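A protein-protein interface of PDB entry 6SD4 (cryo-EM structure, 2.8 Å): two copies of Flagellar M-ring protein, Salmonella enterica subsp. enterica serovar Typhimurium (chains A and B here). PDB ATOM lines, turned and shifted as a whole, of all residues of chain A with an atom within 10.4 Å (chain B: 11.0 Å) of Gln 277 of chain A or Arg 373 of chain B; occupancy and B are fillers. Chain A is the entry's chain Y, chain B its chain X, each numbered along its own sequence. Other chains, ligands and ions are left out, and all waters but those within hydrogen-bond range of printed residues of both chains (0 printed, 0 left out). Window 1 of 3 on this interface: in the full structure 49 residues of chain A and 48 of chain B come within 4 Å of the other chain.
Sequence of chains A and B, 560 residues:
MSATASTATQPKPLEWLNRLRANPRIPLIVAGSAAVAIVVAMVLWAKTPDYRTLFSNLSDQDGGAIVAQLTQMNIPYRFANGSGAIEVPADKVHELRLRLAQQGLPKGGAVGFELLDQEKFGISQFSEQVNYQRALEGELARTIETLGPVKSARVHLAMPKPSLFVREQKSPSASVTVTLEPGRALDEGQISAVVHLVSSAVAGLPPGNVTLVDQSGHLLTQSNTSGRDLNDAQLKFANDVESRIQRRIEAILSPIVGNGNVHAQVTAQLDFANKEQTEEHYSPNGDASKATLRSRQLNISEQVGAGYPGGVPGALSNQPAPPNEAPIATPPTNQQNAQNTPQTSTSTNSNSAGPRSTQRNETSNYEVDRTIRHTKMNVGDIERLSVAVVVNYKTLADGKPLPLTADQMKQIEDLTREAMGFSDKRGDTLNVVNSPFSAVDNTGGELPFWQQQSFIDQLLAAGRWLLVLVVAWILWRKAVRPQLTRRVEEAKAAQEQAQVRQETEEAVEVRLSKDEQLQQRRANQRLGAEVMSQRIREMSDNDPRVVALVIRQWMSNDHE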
ATOM      1  N   ASP A 271      -2.965  10.470  -5.599  1.00  0.00           N
ATOM      2  CA  ASP A 271      -3.812  11.572  -6.036  1.00  0.00           C
ATOM      3  C   ASP A 271      -3.182  12.880  -5.595  1.00  0.00           C
ATOM      4  O   ASP A 271      -3.258  13.245  -4.420  1.00  0.00           O
ATOM      5  CB  ASP A 271      -5.216  11.449  -5.460  1.00  0.00           C
ATOM      6  CG  ASP A 271      -5.827  10.111  -5.721  1.00  0.00           C
ATOM      7  OD1 ASP A 271      -5.680   9.622  -6.855  1.00  0.00           O
ATOM      8  OD2 ASP A 271      -6.472   9.557  -4.807  1.00  0.00           O
ATOM      9  N   ALA A 273      -4.108  15.782  -7.016  1.00  0.00           N
ATOM     10  CA  ALA A 273      -5.018  16.843  -7.406  1.00  0.00           C
ATOM     11  C   ALA A 273      -5.558  17.555  -6.181  1.00  0.00           C
ATOM     12  O   ALA A 273      -6.024  16.920  -5.235  1.00  0.00           O
ATOM     13  CB  ALA A 273      -6.171  16.270  -8.218  1.00  0.00           C
ATOM     14  N   ASN A 274      -5.479  18.879  -6.187  1.00  0.00           N
ATOM     15  CA  ASN A 274      -6.186  19.667  -5.193  1.00  0.00           C
ATOM     16  C   ASN A 274      -7.671  19.480  -5.407  1.00  0.00           C
ATOM     17  O   ASN A 274      -8.110  19.224  -6.523  1.00  0.00           O
ATOM     18  CB  ASN A 274      -5.823  21.136  -5.301  1.00  0.00           C
ATOM     19  CG  ASN A 274      -4.361  21.372  -5.118  1.00  0.00           C
ATOM     20  OD1 ASN A 274      -3.583  21.268  -6.059  1.00  0.00           O
ATOM     21  ND2 ASN A 274      -3.968  21.687  -3.898  1.00  0.00           N
ATOM     22  N   LYS A 275      -8.447  19.591  -4.345  1.00  0.00           N
ATOM     23  CA  LYS A 275      -9.858  19.266  -4.449  1.00  0.00           C
ATOM     24  C   LYS A 275     -10.567  19.785  -3.214  1.00  0.00           C
ATOM     25  O   LYS A 275     -10.201  19.432  -2.097  1.00  0.00           O
ATOM     26  CB  LYS A 275     -10.047  17.776  -4.596  1.00  0.00           C
ATOM     27  CG  LYS A 275     -11.460  17.357  -4.727  1.00  0.00           C
ATOM     28  CD  LYS A 275     -11.497  15.896  -5.009  1.00  0.00           C
ATOM     29  CE  LYS A 275     -10.480  15.540  -6.071  1.00  0.00           C
ATOM     30  NZ  LYS A 275     -10.870  14.336  -6.852  1.00  0.00           N
ATOM     31  N   GLU A 276     -11.560  20.629  -3.422  1.00  0.00           N
ATOM     32  CA  GLU A 276     -12.448  21.069  -2.371  1.00  0.00           C
ATOM     33  C   GLU A 276     -13.831  20.523  -2.641  1.00  0.00           C
ATOM     34  O   GLU A 276     -14.095  19.946  -3.689  1.00  0.00           O
ATOM     35  CB  GLU A 276     -12.482  22.586  -2.283  1.00  0.00           C
ATOM     36  CG  GLU A 276     -11.179  23.158  -1.815  1.00  0.00           C
ATOM     37  CD  GLU A 276     -11.204  24.658  -1.730  1.00  0.00           C
ATOM     38  OE1 GLU A 276     -12.205  25.257  -2.169  1.00  0.00           O
ATOM     39  OE2 GLU A 276     -10.225  25.245  -1.223  1.00  0.00           O
ATOM     40  N   GLN A 277     -14.709  20.689  -1.672  1.00  0.00           N
ATOM     41  CA  GLN A 277     -16.075  20.229  -1.813  1.00  0.00           C
ATOM     42  C   GLN A 277     -16.900  20.945  -0.772  1.00  0.00           C
ATOM     43  O   GLN A 277     -16.357  21.436   0.214  1.00  0.00           O
ATOM     44  CB  GLN A 277     -16.180  18.725  -1.645  1.00  0.00           C
ATOM     45  CG  GLN A 277     -17.472  18.178  -2.116  1.00  0.00           C
ATOM     46  CD  GLN A 277     -17.533  16.707  -1.951  1.00  0.00           C
ATOM     47  OE1 GLN A 277     -16.580  16.093  -1.494  1.00  0.00           O
ATOM     48  NE2 GLN A 277     -18.655  16.117  -2.311  1.00  0.00           N
ATOM     49  N   THR A 278     -18.200  21.036  -1.007  1.00  0.00           N
ATOM     50  CA  THR A 278     -19.108  21.728  -0.105  1.00  0.00           C
ATOM     51  C   THR A 278     -20.504  21.176  -0.320  1.00  0.00           C
ATOM     52  O   THR A 278     -21.275  21.745  -1.089  1.00  0.00           O
ATOM     53  CB  THR A 278     -19.090  23.227  -0.342  1.00  0.00           C
ATOM     54  OG1 THR A 278     -17.743  23.681  -0.462  1.00  0.00           O
ATOM     55  CG2 THR A 278     -19.734  23.943   0.804  1.00  0.00           C
ATOM     56  N   GLU A 279     -20.841  20.087   0.351  1.00  0.00           N
ATOM     57  CA  GLU A 279     -22.231  19.680   0.361  1.00  0.00           C
ATOM     58  C   GLU A 279     -23.070  20.705   1.105  1.00  0.00           C
ATOM     59  O   GLU A 279     -22.555  21.607   1.758  1.00  0.00           O
ATOM     60  CB  GLU A 279     -22.401  18.318   1.011  1.00  0.00           C
ATOM     61  CG  GLU A 279     -21.834  17.172   0.233  1.00  0.00           C
ATOM     62  CD  GLU A 279     -20.365  16.936   0.509  1.00  0.00           C
ATOM     63  OE1 GLU A 279     -19.777  17.662   1.333  1.00  0.00           O
ATOM     64  OE2 GLU A 279     -19.797  16.006  -0.096  1.00  0.00           O
ATOM     65  N   GLU A 280     -24.384  20.560   0.998  1.00  0.00           N
ATOM     66  CA  GLU A 280     -25.300  21.459   1.687  1.00  0.00           C
ATOM     67  C   GLU A 280     -26.659  20.778   1.709  1.00  0.00           C
ATOM     68  O   GLU A 280     -27.616  21.297   1.142  1.00  0.00           O
ATOM     69  CB  GLU A 280     -25.371  22.812   1.010  1.00  0.00           C
ATOM     70  CG  GLU A 280     -26.041  23.868   1.840  1.00  0.00           C
ATOM     71  CD  GLU A 280     -26.574  25.014   1.007  1.00  0.00           C
ATOM     72  OE1 GLU A 280     -26.495  24.938  -0.233  1.00  0.00           O
ATOM     73  OE2 GLU A 280     -27.072  25.999   1.589  1.00  0.00           O
ATOM     74  N   HIS A 281     -26.728  19.630   2.355  1.00  0.00           N
ATOM     75  CA  HIS A 281     -27.938  18.839   2.466  1.00  0.00           C
ATOM     76  C   HIS A 281     -29.024  19.609   3.203  1.00  0.00           C
ATOM     77  O   HIS A 281     -28.743  20.483   4.017  1.00  0.00           O
ATOM     78  CB  HIS A 281     -27.627  17.533   3.189  1.00  0.00           C
ATOM     79  CG  HIS A 281     -28.780  16.586   3.266  1.00  0.00           C
ATOM     80  ND1 HIS A 281     -29.352  16.016   2.151  1.00  0.00           N
ATOM     81  CD2 HIS A 281     -29.457  16.094   4.330  1.00  0.00           C
ATOM     82  CE1 HIS A 281     -30.339  15.221   2.523  1.00  0.00           C
ATOM     83  NE2 HIS A 281     -30.426  15.253   3.840  1.00  0.00           N
ATOM     84  N   ILE A 372     -24.084  21.375   6.457  1.00  0.00           N
ATOM     85  CA  ILE A 372     -23.159  21.998   5.523  1.00  0.00           C
ATOM     86  C   ILE A 372     -21.765  21.476   5.818  1.00  0.00           C
ATOM     87  O   ILE A 372     -21.045  22.065   6.626  1.00  0.00           O
ATOM     88  CB  ILE A 372     -23.173  23.526   5.616  1.00  0.00           C
ATOM     89  CG1 ILE A 372     -24.547  24.081   5.309  1.00  0.00           C
ATOM     90  CG2 ILE A 372     -22.185  24.117   4.651  1.00  0.00           C
ATOM     91  CD1 ILE A 372     -24.552  25.558   5.091  1.00  0.00           C
ATOM     92  N   ARG A 373     -21.370  20.395   5.161  1.00  0.00           N
ATOM     93  CA  ARG A 373     -19.995  19.926   5.211  1.00  0.00           C
ATOM     94  C   ARG A 373     -19.143  20.813   4.325  1.00  0.00           C
ATOM     95  O   ARG A 373     -19.662  21.498   3.451  1.00  0.00           O
ATOM     96  CB  ARG A 373     -19.884  18.478   4.758  1.00  0.00           C
ATOM     97  CG  ARG A 373     -20.736  17.531   5.542  1.00  0.00           C
ATOM     98  CD  ARG A 373     -20.631  16.123   5.015  1.00  0.00           C
ATOM     99  NE  ARG A 373     -19.322  15.521   5.241  1.00  0.00           N
ATOM    100  CZ  ARG A 373     -19.041  14.691   6.240  1.00  0.00           C
ATOM    101  NH1 ARG A 373     -19.975  14.369   7.118  1.00  0.00           N
ATOM    102  NH2 ARG A 373     -17.830  14.179   6.364  1.00  0.00           N
ATOM    103  N   HIS A 374     -17.845  20.813   4.557  1.00  0.00           N
ATOM    104  CA  HIS A 374     -16.906  21.503   3.687  1.00  0.00           C
ATOM    105  C   HIS A 374     -15.556  20.824   3.828  1.00  0.00           C
ATOM    106  O   HIS A 374     -14.764  21.182   4.699  1.00  0.00           O
ATOM    107  CB  HIS A 374     -16.813  22.983   4.022  1.00  0.00           C
ATOM    108  CG  HIS A 374     -15.649  23.666   3.381  1.00  0.00           C
ATOM    109  ND1 HIS A 374     -15.255  23.405   2.088  1.00  0.00           N
ATOM    110  CD2 HIS A 374     -14.784  24.590   3.855  1.00  0.00           C
ATOM    111  CE1 HIS A 374     -14.199  24.139   1.794  1.00  0.00           C
ATOM    112  NE2 HIS A 374     -13.892  24.868   2.849  1.00  0.00           N
ATOM    113  N   THR A 375     -15.296  19.849   2.973  1.00  0.00           N
ATOM    114  CA  THR A 375     -14.057  19.092   2.980  1.00  0.00           C
ATOM    115  C   THR A 375     -13.017  19.809   2.139  1.00  0.00           C
ATOM    116  O   THR A 375     -13.361  20.552   1.223  1.00  0.00           O
ATOM    117  CB  THR A 375     -14.290  17.691   2.432  1.00  0.00           C
ATOM    118  OG1 THR A 375     -15.533  17.192   2.930  1.00  0.00           O
ATOM    119  CG2 THR A 375     -13.192  16.769   2.861  1.00  0.00           C
ATOM    120  N   LYS A 376     -11.760  19.597   2.454  1.00  0.00           N
ATOM    121  CA  LYS A 376     -10.656  19.979   1.591  1.00  0.00           C
ATOM    122  C   LYS A 376      -9.727  18.783   1.531  1.00  0.00           C
ATOM    123  O   LYS A 376      -8.889  18.603   2.414  1.00  0.00           O
ATOM    124  CB  LYS A 376      -9.941  21.217   2.109  1.00  0.00           C
ATOM    125  CG  LYS A 376      -8.711  21.548   1.317  1.00  0.00           C
ATOM    126  CD  LYS A 376      -8.198  22.923   1.635  1.00  0.00           C
ATOM    127  CE  LYS A 376      -6.886  23.190   0.920  1.00  0.00           C
ATOM    128  NZ  LYS A 376      -6.406  24.580   1.149  1.00  0.00           N
ATOM    129  N   MET A 377      -9.880  17.969   0.497  1.00  0.00           N
ATOM    130  CA  MET A 377      -9.255  16.661   0.457  1.00  0.00           C
ATOM    131  C   MET A 377      -7.740  16.764   0.572  1.00  0.00           C
ATOM    132  O   MET A 377      -7.135  17.806   0.327  1.00  0.00           O
ATOM    133  CB  MET A 377      -9.631  15.935  -0.827  1.00  0.00           C
ATOM    134  CG  MET A 377     -11.108  15.966  -1.122  1.00  0.00           C
ATOM    135  SD  MET A 377     -12.038  14.842  -0.079  1.00  0.00           S
ATOM    136  CE  MET A 377     -13.665  15.010  -0.794  1.00  0.00           C
ATOM    137  N   ASN A 378      -7.136  15.648   0.961  1.00  0.00           N
ATOM    138  CA  ASN A 378      -5.700  15.576   1.163  1.00  0.00           C
ATOM    139  C   ASN A 378      -4.996  15.318  -0.160  1.00  0.00           C
ATOM    140  O   ASN A 378      -5.435  14.485  -0.957  1.00  0.00           O
ATOM    141  CB  ASN A 378      -5.368  14.471   2.160  1.00  0.00           C
ATOM    142  CG  ASN A 378      -3.904  14.407   2.490  1.00  0.00           C
ATOM    143  OD1 ASN A 378      -3.292  15.410   2.841  1.00  0.00           O
ATOM    144  ND2 ASN A 378      -3.328  13.222   2.386  1.00  0.00           N
ATOM    145  N   GLU B 276      -8.522  22.900 -14.587  1.00  0.00           N
ATOM    146  CA  GLU B 276      -9.390  23.101 -13.448  1.00  0.00           C
ATOM    147  C   GLU B 276     -10.753  22.530 -13.767  1.00  0.00           C
ATOM    148  O   GLU B 276     -11.027  22.127 -14.892  1.00  0.00           O
ATOM    149  CB  GLU B 276      -9.498  24.575 -13.096  1.00  0.00           C
ATOM    150  CG  GLU B 276      -8.210  25.132 -12.576  1.00  0.00           C
ATOM    151  CD  GLU B 276      -8.310  26.591 -12.229  1.00  0.00           C
ATOM    152  OE1 GLU B 276      -9.357  27.197 -12.527  1.00  0.00           O
ATOM    153  OE2 GLU B 276      -7.343  27.137 -11.658  1.00  0.00           O
ATOM    154  N   GLN B 277     -11.599  22.473 -12.758  1.00  0.00           N
ATOM    155  CA  GLN B 277     -12.943  21.967 -12.936  1.00  0.00           C
ATOM    156  C   GLN B 277     -13.762  22.443 -11.761  1.00  0.00           C
ATOM    157  O   GLN B 277     -13.206  22.788 -10.723  1.00  0.00           O
ATOM    158  CB  GLN B 277     -12.963  20.453 -13.031  1.00  0.00           C
ATOM    159  CG  GLN B 277     -14.242  19.921 -13.549  1.00  0.00           C
ATOM    160  CD  GLN B 277     -14.221  18.443 -13.641  1.00  0.00           C
ATOM    161  OE1 GLN B 277     -13.219  17.815 -13.328  1.00  0.00           O
ATOM    162  NE2 GLN B 277     -15.324  17.859 -14.064  1.00  0.00           N
ATOM    163  N   THR B 278     -15.074  22.496 -11.938  1.00  0.00           N
ATOM    164  CA  THR B 278     -15.980  22.969 -10.902  1.00  0.00           C
ATOM    165  C   THR B 278     -17.352  22.382 -11.167  1.00  0.00           C
ATOM    166  O   THR B 278     -18.182  23.029 -11.801  1.00  0.00           O
ATOM    167  CB  THR B 278     -16.048  24.485 -10.874  1.00  0.00           C
ATOM    168  OG1 THR B 278     -14.733  25.032 -10.953  1.00  0.00           O
ATOM    169  CG2 THR B 278     -16.682  24.955  -9.601  1.00  0.00           C
ATOM    170  N   GLU B 279     -17.605  21.176 -10.687  1.00  0.00           N
ATOM    171  CA  GLU B 279     -18.970  20.693 -10.705  1.00  0.00           C
ATOM    172  C   GLU B 279     -19.830  21.524  -9.768  1.00  0.00           C
ATOM    173  O   GLU B 279     -19.338  22.329  -8.984  1.00  0.00           O
ATOM    174  CB  GLU B 279     -19.044  19.233 -10.298  1.00  0.00           C
ATOM    175  CG  GLU B 279     -18.448  18.272 -11.281  1.00  0.00           C
ATOM    176  CD  GLU B 279     -16.959  18.079 -11.095  1.00  0.00           C
ATOM    177  OE1 GLU B 279     -16.378  18.684 -10.174  1.00  0.00           O
ATOM    178  OE2 GLU B 279     -16.368  17.301 -11.869  1.00  0.00           O
ATOM    179  N   GLU B 280     -21.138  21.324  -9.859  1.00  0.00           N
ATOM    180  CA  GLU B 280     -22.072  22.035  -8.995  1.00  0.00           C
ATOM    181  C   GLU B 280     -23.392  21.283  -9.053  1.00  0.00           C
ATOM    182  O   GLU B 280     -24.397  21.835  -9.490  1.00  0.00           O
ATOM    183  CB  GLU B 280     -22.240  23.478  -9.425  1.00  0.00           C
ATOM    184  CG  GLU B 280     -22.930  24.335  -8.404  1.00  0.00           C
ATOM    185  CD  GLU B 280     -23.556  25.573  -9.007  1.00  0.00           C
ATOM    186  OE1 GLU B 280     -23.522  25.717 -10.243  1.00  0.00           O
ATOM    187  OE2 GLU B 280     -24.080  26.412  -8.247  1.00  0.00           O
ATOM    188  N   HIS B 281     -23.374  20.038  -8.615  1.00  0.00           N
ATOM    189  CA  HIS B 281     -24.537  19.170  -8.607  1.00  0.00           C
ATOM    190  C   HIS B 281     -25.631  19.738  -7.714  1.00  0.00           C
ATOM    191  O   HIS B 281     -25.363  20.472  -6.769  1.00  0.00           O
ATOM    192  CB  HIS B 281     -24.129  17.780  -8.131  1.00  0.00           C
ATOM    193  CG  HIS B 281     -25.226  16.768  -8.187  1.00  0.00           C
ATOM    194  ND1 HIS B 281     -25.813  16.367  -9.367  1.00  0.00           N
ATOM    195  CD2 HIS B 281     -25.835  16.062  -7.204  1.00  0.00           C
ATOM    196  CE1 HIS B 281     -26.742  15.464  -9.108  1.00  0.00           C
ATOM    197  NE2 HIS B 281     -26.778  15.264  -7.804  1.00  0.00           N
ATOM    198  N   TYR B 282     -26.871  19.416  -8.043  1.00  0.00           N
ATOM    199  CA  TYR B 282     -28.022  19.715  -7.209  1.00  0.00           C
ATOM    200  C   TYR B 282     -28.783  18.422  -7.006  1.00  0.00           C
ATOM    201  O   TYR B 282     -28.576  17.458  -7.741  1.00  0.00           O
ATOM    202  CB  TYR B 282     -28.938  20.750  -7.839  1.00  0.00           C
ATOM    203  CG  TYR B 282     -28.466  22.159  -7.687  1.00  0.00           C
ATOM    204  CD1 TYR B 282     -28.979  22.974  -6.710  1.00  0.00           C
ATOM    205  CD2 TYR B 282     -27.504  22.672  -8.516  1.00  0.00           C
ATOM    206  CE1 TYR B 282     -28.544  24.253  -6.569  1.00  0.00           C
ATOM    207  CE2 TYR B 282     -27.065  23.947  -8.382  1.00  0.00           C
ATOM    208  CZ  TYR B 282     -27.588  24.737  -7.409  1.00  0.00           C
ATOM    209  OH  TYR B 282     -27.145  26.022  -7.272  1.00  0.00           O
ATOM    210  N   SER B 283     -29.636  18.393  -6.042  1.00  0.00           N
ATOM    211  CA  SER B 283     -30.337  17.133  -5.869  1.00  0.00           C
ATOM    212  C   SER B 283     -31.772  17.259  -6.361  1.00  0.00           C
ATOM    213  O   SER B 283     -32.447  18.241  -6.057  1.00  0.00           O
ATOM    214  CB  SER B 283     -30.325  16.700  -4.413  1.00  0.00           C
ATOM    215  OG  SER B 283     -29.022  16.347  -4.005  1.00  0.00           O
ATOM    216  N   ASP B 369     -30.506  20.857  -2.068  1.00  0.00           N
ATOM    217  CA  ASP B 369     -29.208  20.354  -1.649  1.00  0.00           C
ATOM    218  C   ASP B 369     -28.203  20.544  -2.766  1.00  0.00           C
ATOM    219  O   ASP B 369     -28.454  20.170  -3.907  1.00  0.00           O
ATOM    220  CB  ASP B 369     -29.290  18.876  -1.297  1.00  0.00           C
ATOM    221  CG  ASP B 369     -30.547  18.527  -0.562  1.00  0.00           C
ATOM    222  OD1 ASP B 369     -31.292  19.450  -0.198  1.00  0.00           O
ATOM    223  OD2 ASP B 369     -30.786  17.331  -0.324  1.00  0.00           O
ATOM    224  N   ARG B 370     -27.049  21.103  -2.440  1.00  0.00           N
ATOM    225  CA  ARG B 370     -26.111  21.498  -3.476  1.00  0.00           C
ATOM    226  C   ARG B 370     -24.693  21.122  -3.088  1.00  0.00           C
ATOM    227  O   ARG B 370     -24.157  21.668  -2.126  1.00  0.00           O
ATOM    228  CB  ARG B 370     -26.200  22.989  -3.719  1.00  0.00           C
ATOM    229  CG  ARG B 370     -25.086  23.485  -4.561  1.00  0.00           C
ATOM    230  CD  ARG B 370     -25.185  24.948  -4.756  1.00  0.00           C
ATOM    231  NE  ARG B 370     -24.970  25.658  -3.516  1.00  0.00           N
ATOM    232  CZ  ARG B 370     -24.434  26.864  -3.448  1.00  0.00           C
ATOM    233  NH1 ARG B 370     -24.062  27.479  -4.560  1.00  0.00           N
ATOM    234  NH2 ARG B 370     -24.270  27.455  -2.276  1.00  0.00           N
ATOM    235  N   THR B 371     -24.078  20.229  -3.851  1.00  0.00           N
ATOM    236  CA  THR B 371     -22.655  19.951  -3.749  1.00  0.00           C
ATOM    237  C   THR B 371     -21.890  20.844  -4.710  1.00  0.00           C
ATOM    238  O   THR B 371     -22.406  21.212  -5.760  1.00  0.00           O
ATOM    239  CB  THR B 371     -22.365  18.493  -4.072  1.00  0.00           C
ATOM    240  OG1 THR B 371     -23.299  17.663  -3.384  1.00  0.00           O
ATOM    241  CG2 THR B 371     -20.982  18.127  -3.636  1.00  0.00           C
ATOM    242  N   ILE B 372     -20.662  21.200  -4.353  1.00  0.00           N
ATOM    243  CA  ILE B 372     -19.809  22.028  -5.192  1.00  0.00           C
ATOM    244  C   ILE B 372     -18.380  21.545  -5.036  1.00  0.00           C
ATOM    245  O   ILE B 372     -17.659  22.027  -4.159  1.00  0.00           O
ATOM    246  CB  ILE B 372     -19.900  23.514  -4.833  1.00  0.00           C
ATOM    247  CG1 ILE B 372     -21.312  24.032  -4.998  1.00  0.00           C
ATOM    248  CG2 ILE B 372     -18.983  24.319  -5.711  1.00  0.00           C
ATOM    249  CD1 ILE B 372     -21.403  25.522  -4.953  1.00  0.00           C
ATOM    250  N   ARG B 373     -17.956  20.619  -5.883  1.00  0.00           N
ATOM    251  CA  ARG B 373     -16.557  20.230  -5.957  1.00  0.00           C
ATOM    252  C   ARG B 373     -15.789  21.304  -6.699  1.00  0.00           C
ATOM    253  O   ARG B 373     -16.378  22.098  -7.425  1.00  0.00           O
ATOM    254  CB  ARG B 373     -16.390  18.889  -6.658  1.00  0.00           C
ATOM    255  CG  ARG B 373     -17.160  17.774  -6.027  1.00  0.00           C
ATOM    256  CD  ARG B 373     -17.003  16.487  -6.794  1.00  0.00           C
ATOM    257  NE  ARG B 373     -15.655  15.931  -6.716  1.00  0.00           N
ATOM    258  CZ  ARG B 373     -15.292  14.959  -5.885  1.00  0.00           C
ATOM    259  NH1 ARG B 373     -16.171  14.437  -5.049  1.00  0.00           N
ATOM    260  NH2 ARG B 373     -14.052  14.505  -5.890  1.00  0.00           N
ATOM    261  N   HIS B 374     -14.485  21.340  -6.511  1.00  0.00           N
ATOM    262  CA  HIS B 374     -13.617  22.223  -7.275  1.00  0.00           C
ATOM    263  C   HIS B 374     -12.230  21.609  -7.296  1.00  0.00           C
ATOM    264  O   HIS B 374     -11.424  21.857  -6.400  1.00  0.00           O
ATOM    265  CB  HIS B 374     -13.590  23.626  -6.691  1.00  0.00           C
ATOM    266  CG  HIS B 374     -12.490  24.475  -7.239  1.00  0.00           C
ATOM    267  ND1 HIS B 374     -12.133  24.464  -8.567  1.00  0.00           N
ATOM    268  CD2 HIS B 374     -11.655  25.352  -6.636  1.00  0.00           C
ATOM    269  CE1 HIS B 374     -11.129  25.299  -8.762  1.00  0.00           C
ATOM    270  NE2 HIS B 374     -10.820  25.851  -7.605  1.00  0.00           N
ATOM    271  N   THR B 375     -11.954  20.813  -8.316  1.00  0.00           N
ATOM    272  CA  THR B 375     -10.679  20.141  -8.479  1.00  0.00           C
ATOM    273  C   THR B 375      -9.711  21.051  -9.213  1.00  0.00           C
ATOM    274  O   THR B 375     -10.129  21.919  -9.974  1.00  0.00           O
ATOM    275  CB  THR B 375     -10.859  18.842  -9.255  1.00  0.00           C
ATOM    276  OG1 THR B 375     -12.053  18.194  -8.814  1.00  0.00           O
ATOM    277  CG2 THR B 375      -9.699  17.927  -9.027  1.00  0.00           C
ATOM    278  N   LYS B 376      -8.434  20.860  -8.978  1.00  0.00           N
ATOM    279  CA  LYS B 376      -7.386  21.450  -9.794  1.00  0.00           C
ATOM    280  C   LYS B 376      -6.399  20.338 -10.089  1.00  0.00           C
ATOM    281  O   LYS B 376      -5.518  20.057  -9.278  1.00  0.00           O
ATOM    282  CB  LYS B 376      -6.717  22.619  -9.091  1.00  0.00           C
ATOM    283  CG  LYS B 376      -5.538  23.153  -9.850  1.00  0.00           C
ATOM    284  CD  LYS B 376      -5.086  24.481  -9.312  1.00  0.00           C
ATOM    285  CE  LYS B 376      -3.818  24.943 -10.009  1.00  0.00           C
ATOM    286  NZ  LYS B 376      -3.403  26.298  -9.556  1.00  0.00           N
ATOM    287  N   MET B 377      -6.550  19.707 -11.245  1.00  0.00           N
ATOM    288  CA  MET B 377      -5.861  18.465 -11.532  1.00  0.00           C
ATOM    289  C   MET B 377      -4.351  18.633 -11.446  1.00  0.00           C
ATOM    290  O   MET B 377      -3.810  19.736 -11.524  1.00  0.00           O
ATOM    291  CB  MET B 377      -6.249  17.950 -12.911  1.00  0.00           C
ATOM    292  CG  MET B 377      -7.737  17.945 -13.151  1.00  0.00           C
ATOM    293  SD  MET B 377      -8.565  16.606 -12.292  1.00  0.00           S
ATOM    294  CE  MET B 377     -10.226  16.799 -12.918  1.00  0.00           C
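The side-chain carboxylate (OD2) of Asp 369 of chain B lies within hydrogen-bond range of a ring nitrogen (ND1) of His 281 of chain A (3.1 Å). The side-chain carboxylate (OE1) of Glu 280 of chain A lies within salt-bridge range of the guanidinium group (NE) of Arg 370 of chain B. The backbone NH (N) of Thr 278 of chain A is in hydrogen-bond range of the backbone carbonyl oxygen (O) of Ile 372 of chain B, at 3.3 Å. N of His 374 of chain B sits at hydrogen-bond distance from O of Glu 276 of chain A (3.2 Å). The backbone NH of Lys 376 of chain B sits at hydrogen-bond distance from the backbone carbonyl oxygen of Asn 274 of chain A (3.0 Å). The side-chain amino group of Lys 275 of chain A sits close to the guanidinium group of Arg 373 of chain B (3.3 Å). O of Thr 278 of chain A sits close to O of Arg 370 of chain B (3.1 Å).
O of Gln 277 of chain B sits at hydrogen-bond distance from ND1 of His 374 of chain B (2.9 Å). The backbone NH (N) of Gln 277 of chain B is in hydrogen-bond range of the backbone carbonyl oxygen (O) of Thr 375 of chain B, 3.2 Å away. The side-chain amide nitrogen of Gln 277 of chain A lies within hydrogen-bond range of the side-chain carboxylate of Glu 279 of chain A (2.5 Å).
Ala 273 of chain A touches Lys 376 of chain B. Lys 275 of chain A touches His 374 of chain B (CA to O, 3.6 Å). Lys 275 of chain A touches Thr 375 of chain B. NE2 of Gln 277 of chain A touches CG2 of Thr 371 of chain B, at 3.3 Å. Gln 277 of chain A touches Ile 372 of chain B. Gln 277 of chain A touches Arg 373 of chain B. Glu 279 of chain A touches Arg 370 of chain B.
Glu 276 of chain A touches just these residues of chain B: Arg 373 and His 374. Glu 279 of chain A touches just these residues of chain B: Arg 370 and Thr 371. His 374 of chain A touches none of the printed residues of chain B. No residue of chain B comes within 4 Å of Thr 375 of chain A. No residue of chain A comes within 4 Å of Glu 279 of chain B. Of the printed residues of chain A, Thr 371 of chain B touches Gln 277, Thr 278 and Glu 279. Printed residues of chain A within 4 Å of Lys 376 of chain B: Ala 273 and Asn 274. The nearest residue of chain A that does not touch Arg 373 of chain B is Thr 278 of chain A (4.9 Å).
Of the 17 printed residues of chain B, 9 touch a printed residue of chain A. Hydrophobic or aromatic side chains of chain A that line the printed part of chain B: Ala 273 and His 281. Among the printed residues, 21 pairs touch across the chains. Among the printed residues, Asp or Glu carboxylates within 4 Å of a Lys or Arg side-chain nitrogen of the other chain: Glu 280 of chain A with Arg 370 of chain B.
Gln 277 of chain A touches Arg 373 of chain B, but with the chains exchanged Arg 373 of chain A does not touch Gln 277 of chain B (15.6 Å). Thr 278 of chain A touches Ile 372 of chain B, but with the chains exchanged Ile 372 of chain A does not touch Thr 278 of chain B (15.3 Å). Positions printed for both chains: 276, 277, 278, 279, 280, 281, 372, 373, 374, 375, 376 and 377.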
